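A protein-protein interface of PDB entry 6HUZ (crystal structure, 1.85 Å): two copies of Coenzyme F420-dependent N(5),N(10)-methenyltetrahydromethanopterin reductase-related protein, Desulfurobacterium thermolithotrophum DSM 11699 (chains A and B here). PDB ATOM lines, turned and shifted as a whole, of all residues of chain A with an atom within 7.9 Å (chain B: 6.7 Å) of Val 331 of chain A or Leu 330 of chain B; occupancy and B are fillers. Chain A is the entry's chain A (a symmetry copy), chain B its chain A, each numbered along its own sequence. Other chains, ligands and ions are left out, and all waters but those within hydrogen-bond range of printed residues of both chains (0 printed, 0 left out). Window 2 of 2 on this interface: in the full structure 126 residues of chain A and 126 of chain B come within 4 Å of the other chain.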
ATOM      1  N   VAL A 324      20.563 -14.116   2.067  1.00  0.00           N
ATOM      2  CA  VAL A 324      21.342 -14.102   3.310  1.00  0.00           C
ATOM      3  C   VAL A 324      21.772 -15.547   3.657  1.00  0.00           C
ATOM      4  O   VAL A 324      22.951 -15.796   3.946  1.00  0.00           O
ATOM      5  CB  VAL A 324      20.578 -13.402   4.468  1.00  0.00           C
ATOM      6  CG1 VAL A 324      21.246 -13.661   5.836  1.00  0.00           C
ATOM      7  CG2 VAL A 324      20.498 -11.898   4.217  1.00  0.00           C
ATOM      8  N   GLU A 325      20.839 -16.501   3.592  1.00  0.00           N
ATOM      9  CA  GLU A 325      21.152 -17.894   3.911  1.00  0.00           C
ATOM     10  C   GLU A 325      22.238 -18.457   2.989  1.00  0.00           C
ATOM     11  O   GLU A 325      23.136 -19.131   3.461  1.00  0.00           O
ATOM     12  CB  GLU A 325      19.899 -18.777   3.784  1.00  0.00           C
ATOM     13  CG  GLU A 325      19.007 -18.729   5.007  1.00  0.00           C
ATOM     14  CD  GLU A 325      17.680 -19.434   4.815  1.00  0.00           C
ATOM     15  OE1 GLU A 325      16.628 -18.786   5.026  1.00  0.00           O
ATOM     16  OE2 GLU A 325      17.687 -20.633   4.451  1.00  0.00           O
ATOM     17  N   HIS A 326      22.133 -18.196   1.696  1.00  0.00           N
ATOM     18  CA  HIS A 326      23.095 -18.675   0.706  1.00  0.00           C
ATOM     19  C   HIS A 326      24.464 -18.058   0.947  1.00  0.00           C
ATOM     20  O   HIS A 326      25.473 -18.766   0.910  1.00  0.00           O
ATOM     21  CB  HIS A 326      22.624 -18.334  -0.714  1.00  0.00           C
ATOM     22  CG  HIS A 326      21.709 -19.364  -1.304  1.00  0.00           C
ATOM     23  ND1 HIS A 326      20.329 -19.286  -1.146  1.00  0.00           N
ATOM     24  CD2 HIS A 326      22.000 -20.468  -2.026  1.00  0.00           C
ATOM     25  CE1 HIS A 326      19.830 -20.337  -1.780  1.00  0.00           C
ATOM     26  NE2 HIS A 326      20.799 -21.074  -2.331  1.00  0.00           N
ATOM     27  N   MET A 327      24.500 -16.738   1.166  1.00  0.00           N
ATOM     28  CA  MET A 327      25.750 -16.025   1.432  1.00  0.00           C
ATOM     29  C   MET A 327      26.420 -16.564   2.693  1.00  0.00           C
ATOM     30  O   MET A 327      27.627 -16.830   2.674  1.00  0.00           O
ATOM     31  CB  MET A 327      25.491 -14.526   1.587  1.00  0.00           C
ATOM     32  CG  MET A 327      25.404 -13.822   0.273  1.00  0.00           C
ATOM     33  SD  MET A 327      27.014 -13.837  -0.561  1.00  0.00           S
ATOM     34  CE  MET A 327      27.738 -12.422   0.214  1.00  0.00           C
ATOM     35  N   GLU A 328      25.643 -16.751   3.779  1.00  0.00           N
ATOM     36  CA  GLU A 328      26.180 -17.294   5.036  1.00  0.00           C
ATOM     37  C   GLU A 328      26.803 -18.683   4.790  1.00  0.00           C
ATOM     38  O   GLU A 328      27.843 -18.990   5.360  1.00  0.00           O
ATOM     39  CB  GLU A 328      25.080 -17.445   6.108  1.00  0.00           C
ATOM     40  CG  GLU A 328      24.643 -16.150   6.772  1.00  0.00           C
ATOM     41  CD  GLU A 328      25.629 -15.521   7.734  1.00  0.00           C
ATOM     42  OE1 GLU A 328      26.666 -16.153   8.035  1.00  0.00           O
ATOM     43  OE2 GLU A 328      25.368 -14.385   8.184  1.00  0.00           O
ATOM     44  N   ASP A 329      26.150 -19.521   3.959  1.00  0.00           N
ATOM     45  CA  ASP A 329      26.640 -20.876   3.648  1.00  0.00           C
ATOM     46  C   ASP A 329      27.888 -20.843   2.771  1.00  0.00           C
ATOM     47  O   ASP A 329      28.762 -21.690   2.901  1.00  0.00           O
ATOM     48  CB  ASP A 329      25.556 -21.689   2.906  1.00  0.00           C
ATOM     49  CG  ASP A 329      24.410 -22.173   3.772  1.00  0.00           C
ATOM     50  OD1 ASP A 329      24.584 -22.238   5.011  1.00  0.00           O
ATOM     51  OD2 ASP A 329      23.342 -22.483   3.213  1.00  0.00           O
ATOM     52  N   LEU A 330      27.955 -19.879   1.863  1.00  0.00           N
ATOM     53  CA  LEU A 330      29.066 -19.725   0.924  1.00  0.00           C
ATOM     54  C   LEU A 330      30.312 -19.018   1.523  1.00  0.00           C
ATOM     55  O   LEU A 330      31.443 -19.502   1.384  1.00  0.00           O
ATOM     56  CB  LEU A 330      28.500 -18.912  -0.260  1.00  0.00           C
ATOM     57  CG  LEU A 330      29.384 -18.710  -1.473  1.00  0.00           C
ATOM     58  CD1 LEU A 330      29.860 -20.038  -2.044  1.00  0.00           C
ATOM     59  CD2 LEU A 330      28.625 -17.961  -2.545  1.00  0.00           C
ATOM     60  N   VAL A 331      30.125 -17.898   2.202  1.00  0.00           N
ATOM     61  CA  VAL A 331      31.277 -17.166   2.738  1.00  0.00           C
ATOM     62  C   VAL A 331      31.325 -16.953   4.234  1.00  0.00           C
ATOM     63  O   VAL A 331      32.355 -16.487   4.716  1.00  0.00           O
ATOM     64  CB  VAL A 331      31.424 -15.801   2.012  1.00  0.00           C
ATOM     65  CG1 VAL A 331      31.783 -15.999   0.544  1.00  0.00           C
ATOM     66  CG2 VAL A 331      30.152 -14.962   2.135  1.00  0.00           C
ATOM     67  N   GLY A 332      30.263 -17.272   4.968  1.00  0.00           N
ATOM     68  CA  GLY A 332      30.271 -17.064   6.410  1.00  0.00           C
ATOM     69  C   GLY A 332      29.794 -15.679   6.793  1.00  0.00           C
ATOM     70  O   GLY A 332      29.683 -14.789   5.944  1.00  0.00           O
ATOM     71  N   ASP A 333      29.526 -15.504   8.093  1.00  0.00           N
ATOM     72  CA  ASP A 333      28.985 -14.281   8.696  1.00  0.00           C
ATOM     73  C   ASP A 333      29.820 -13.045   8.681  1.00  0.00           C
ATOM     74  O   ASP A 333      29.295 -11.966   8.393  1.00  0.00           O
ATOM     75  CB  ASP A 333      28.590 -14.532  10.153  1.00  0.00           C
ATOM     76  CG  ASP A 333      27.667 -13.447  10.645  1.00  0.00           C
ATOM     77  OD1 ASP A 333      26.572 -13.301  10.077  1.00  0.00           O
ATOM     78  OD2 ASP A 333      28.049 -12.727  11.577  1.00  0.00           O
ATOM     79  N   ASP A 334      31.094 -13.178   9.049  1.00  0.00           N
ATOM     80  CA  ASP A 334      32.005 -12.040   9.102  1.00  0.00           C
ATOM     81  C   ASP A 334      32.037 -11.435   7.730  1.00  0.00           C
ATOM     82  O   ASP A 334      31.891 -10.223   7.579  1.00  0.00           O
ATOM     83  CB  ASP A 334      33.415 -12.479   9.544  1.00  0.00           C
ATOM     84  CG  ASP A 334      33.395 -13.546  10.623  1.00  0.00           C
ATOM     85  OD1 ASP A 334      33.303 -13.183  11.818  1.00  0.00           O
ATOM     86  OD2 ASP A 334      33.459 -14.750  10.270  1.00  0.00           O
ATOM     87  N   VAL A 335      32.177 -12.289   6.716  1.00  0.00           N
ATOM     88  CA  VAL A 335      32.206 -11.822   5.335  1.00  0.00           C
ATOM     89  C   VAL A 335      30.872 -11.174   4.994  1.00  0.00           C
ATOM     90  O   VAL A 335      30.848 -10.147   4.320  1.00  0.00           O
ATOM     91  CB  VAL A 335      32.601 -12.953   4.362  1.00  0.00           C
ATOM     92  CG1 VAL A 335      32.560 -12.461   2.917  1.00  0.00           C
ATOM     93  CG2 VAL A 335      33.990 -13.489   4.710  1.00  0.00           C
ATOM     94  N   LEU A 336      29.759 -11.748   5.482  1.00  0.00           N
ATOM     95  CA  LEU A 336      28.436 -11.181   5.218  1.00  0.00           C
ATOM     96  C   LEU A 336      28.201  -9.880   5.992  1.00  0.00           C
ATOM     97  O   LEU A 336      27.540  -9.003   5.462  1.00  0.00           O
ATOM     98  CB  LEU A 336      27.327 -12.220   5.499  1.00  0.00           C
ATOM     99  CG  LEU A 336      25.894 -11.772   5.225  1.00  0.00           C
ATOM    100  CD1 LEU A 336      25.746 -11.155   3.856  1.00  0.00           C
ATOM    101  CD2 LEU A 336      24.967 -12.899   5.361  1.00  0.00           C
ATOM    102  N   LYS A 337      28.745  -9.743   7.236  1.00  0.00           N
ATOM    103  CA  LYS A 337      28.618  -8.533   8.074  1.00  0.00           C
ATOM    104  C   LYS A 337      29.241  -7.287   7.403  1.00  0.00           C
ATOM    105  O   LYS A 337      28.810  -6.167   7.669  1.00  0.00           O
ATOM    106  CB  LYS A 337      29.268  -8.727   9.464  1.00  0.00           C
ATOM    107  CG  LYS A 337      28.390  -9.503  10.435  1.00  0.00           C
ATOM    108  CD  LYS A 337      28.632  -9.119  11.887  1.00  0.00           C
ATOM    109  CE  LYS A 337      27.351  -8.857  12.650  1.00  0.00           C
ATOM    110  NZ  LYS A 337      26.614 -10.115  12.956  1.00  0.00           N
ATOM    111  N   ILE A 339      28.606  -6.028   4.840  1.00  0.00           N
ATOM    112  CA  ILE A 339      27.561  -5.570   3.910  1.00  0.00           C
ATOM    113  C   ILE A 339      26.545  -4.691   4.681  1.00  0.00           C
ATOM    114  O   ILE A 339      26.157  -3.614   4.220  1.00  0.00           O
ATOM    115  CB  ILE A 339      26.876  -6.777   3.247  1.00  0.00           C
ATOM    116  CG1 ILE A 339      27.701  -7.300   2.043  1.00  0.00           C
ATOM    117  CG2 ILE A 339      25.454  -6.410   2.804  1.00  0.00           C
ATOM    118  CD1 ILE A 339      29.037  -8.012   2.372  1.00  0.00           C
ATOM    119  N   GLU B 325      24.183  -7.913  -6.043  1.00  0.00           N
ATOM    120  CA  GLU B 325      25.427  -7.488  -6.685  1.00  0.00           C
ATOM    121  C   GLU B 325      26.617  -8.342  -6.236  1.00  0.00           C
ATOM    122  O   GLU B 325      27.425  -8.729  -7.061  1.00  0.00           O
ATOM    123  CB  GLU B 325      25.733  -6.016  -6.362  1.00  0.00           C
ATOM    124  CG  GLU B 325      24.981  -5.042  -7.244  1.00  0.00           C
ATOM    125  CD  GLU B 325      25.121  -3.598  -6.805  1.00  0.00           C
ATOM    126  OE1 GLU B 325      24.077  -2.942  -6.582  1.00  0.00           O
ATOM    127  OE2 GLU B 325      26.273  -3.120  -6.682  1.00  0.00           O
ATOM    128  N   HIS B 326      26.724  -8.603  -4.942  1.00  0.00           N
ATOM    129  CA  HIS B 326      27.811  -9.399  -4.377  1.00  0.00           C
ATOM    130  C   HIS B 326      27.750 -10.829  -4.890  1.00  0.00           C
ATOM    131  O   HIS B 326      28.779 -11.390  -5.275  1.00  0.00           O
ATOM    132  CB  HIS B 326      27.739  -9.402  -2.845  1.00  0.00           C
ATOM    133  CG  HIS B 326      28.441  -8.240  -2.211  1.00  0.00           C
ATOM    134  ND1 HIS B 326      27.778  -7.047  -1.945  1.00  0.00           N
ATOM    135  CD2 HIS B 326      29.727  -8.117  -1.816  1.00  0.00           C
ATOM    136  CE1 HIS B 326      28.677  -6.245  -1.394  1.00  0.00           C
ATOM    137  NE2 HIS B 326      29.864  -6.849  -1.290  1.00  0.00           N
ATOM    138  N   MET B 327      26.553 -11.427  -4.868  1.00  0.00           N
ATOM    139  CA  MET B 327      26.353 -12.794  -5.352  1.00  0.00           C
ATOM    140  C   MET B 327      26.723 -12.902  -6.829  1.00  0.00           C
ATOM    141  O   MET B 327      27.441 -13.833  -7.209  1.00  0.00           O
ATOM    142  CB  MET B 327      24.901 -13.228  -5.152  1.00  0.00           C
ATOM    143  CG  MET B 327      24.635 -13.712  -3.765  1.00  0.00           C
ATOM    144  SD  MET B 327      25.531 -15.257  -3.450  1.00  0.00           S
ATOM    145  CE  MET B 327      24.363 -16.396  -4.134  1.00  0.00           C
ATOM    146  N   GLU B 328      26.261 -11.943  -7.658  1.00  0.00           N
ATOM    147  CA  GLU B 328      26.583 -11.935  -9.093  1.00  0.00           C
ATOM    148  C   GLU B 328      28.111 -11.884  -9.293  1.00  0.00           C
ATOM    149  O   GLU B 328      28.628 -12.546 -10.186  1.00  0.00           O
ATOM    150  CB  GLU B 328      25.964 -10.715  -9.808  1.00  0.00           C
ATOM    151  CG  GLU B 328      24.471 -10.810 -10.072  1.00  0.00           C
ATOM    152  CD  GLU B 328      24.039 -11.782 -11.148  1.00  0.00           C
ATOM    153  OE1 GLU B 328      24.914 -12.340 -11.846  1.00  0.00           O
ATOM    154  OE2 GLU B 328      22.815 -11.995 -11.290  1.00  0.00           O
ATOM    155  N   ASP B 329      28.821 -11.082  -8.474  1.00  0.00           N
ATOM    156  CA  ASP B 329      30.286 -10.943  -8.568  1.00  0.00           C
ATOM    157  C   ASP B 329      31.008 -12.202  -8.100  1.00  0.00           C
ATOM    158  O   ASP B 329      32.056 -12.550  -8.629  1.00  0.00           O
ATOM    159  CB  ASP B 329      30.776  -9.761  -7.703  1.00  0.00           C
ATOM    160  CG  ASP B 329      30.489  -8.386  -8.271  1.00  0.00           C
ATOM    161  OD1 ASP B 329      30.255  -8.283  -9.499  1.00  0.00           O
ATOM    162  OD2 ASP B 329      30.495  -7.414  -7.493  1.00  0.00           O
ATOM    163  N   LEU B 330      30.460 -12.866  -7.092  1.00  0.00           N
ATOM    164  CA  LEU B 330      31.041 -14.073  -6.504  1.00  0.00           C
ATOM    165  C   LEU B 330      30.749 -15.373  -7.301  1.00  0.00           C
ATOM    166  O   LEU B 330      31.661 -16.161  -7.586  1.00  0.00           O
ATOM    167  CB  LEU B 330      30.452 -14.167  -5.080  1.00  0.00           C
ATOM    168  CG  LEU B 330      30.980 -15.248  -4.160  1.00  0.00           C
ATOM    169  CD1 LEU B 330      32.492 -15.156  -4.001  1.00  0.00           C
ATOM    170  CD2 LEU B 330      30.337 -15.125  -2.797  1.00  0.00           C
ATOM    171  N   VAL B 331      29.502 -15.602  -7.683  1.00  0.00           N
ATOM    172  CA  VAL B 331      29.170 -16.843  -8.389  1.00  0.00           C
ATOM    173  C   VAL B 331      28.570 -16.713  -9.770  1.00  0.00           C
ATOM    174  O   VAL B 331      28.435 -17.735 -10.438  1.00  0.00           O
ATOM    175  CB  VAL B 331      28.252 -17.728  -7.503  1.00  0.00           C
ATOM    176  CG1 VAL B 331      28.992 -18.215  -6.263  1.00  0.00           C
ATOM    177  CG2 VAL B 331      26.979 -16.984  -7.097  1.00  0.00           C
ATOM    178  N   GLY B 332      28.211 -15.509 -10.210  1.00  0.00           N
ATOM    179  CA  GLY B 332      27.615 -15.352 -11.529  1.00  0.00           C
ATOM    180  C   GLY B 332      26.109 -15.503 -11.501  1.00  0.00           C
ATOM    181  O   GLY B 332      25.536 -15.968 -10.510  1.00  0.00           O
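Of the 15 printed residues of chain A, 4 touch a printed residue of chain B. Hydrophobic or aromatic side chains of chain A within 4 Å of the printed part of chain B: Met 327, Leu 330, Val 331 and Ile 339. Among the printed residues, 5 pairs touch across the chains. Among the printed residues, no Asp or Glu carboxylate lies within 4 Å of a Lys or Arg side-chain nitrogen of the other chain.
Val 331 of chain A touches just one residue of chain B: Leu 330. Of the printed residues of chain A, Leu 330 of chain B touches Leu 330 (3.3 Å) and Val 331 (3.7 Å). Of the printed residues of chain A, His 326 of chain B touches Ile 339. Printed residues of chain B within 4 Å of Ile 339 of chain A: His 326. Printed residues of chain A within 4 Å of Val 331 of chain B: Leu 330. Printed residues of chain B within 4 Å of Met 327 of chain A: Met 327 (3.5 Å).
Met 327 of chain B touches its own counterpart, Met 327 of chain A. Leu 330 of chain B touches its own counterpart, Leu 330 of chain A. Leu 330 of chain A touches Val 331 of chain B, and with the chains exchanged Val 331 of chain A touches Leu 330 of chain B. Of the 5 pairs that touch across the chains among the printed residues, 4 have their exchanged pair printed and touching as well.
The side-chain sulfur (SD) of Met 327 of chain A sits close to the side-chain sulfur (SD) of Met 327 of chain B (3.5 Å).
Leu 330 of chain A touches Leu 330 of chain B. CD2 of Leu 330 of chain A touches CG1 of Val 331 of chain B, at 3.7 Å. Val 331 of chain A touches Leu 330 of chain B. CG1 of Ile 339 of chain A touches CE1 of His 326 of chain B (3.7 Å).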
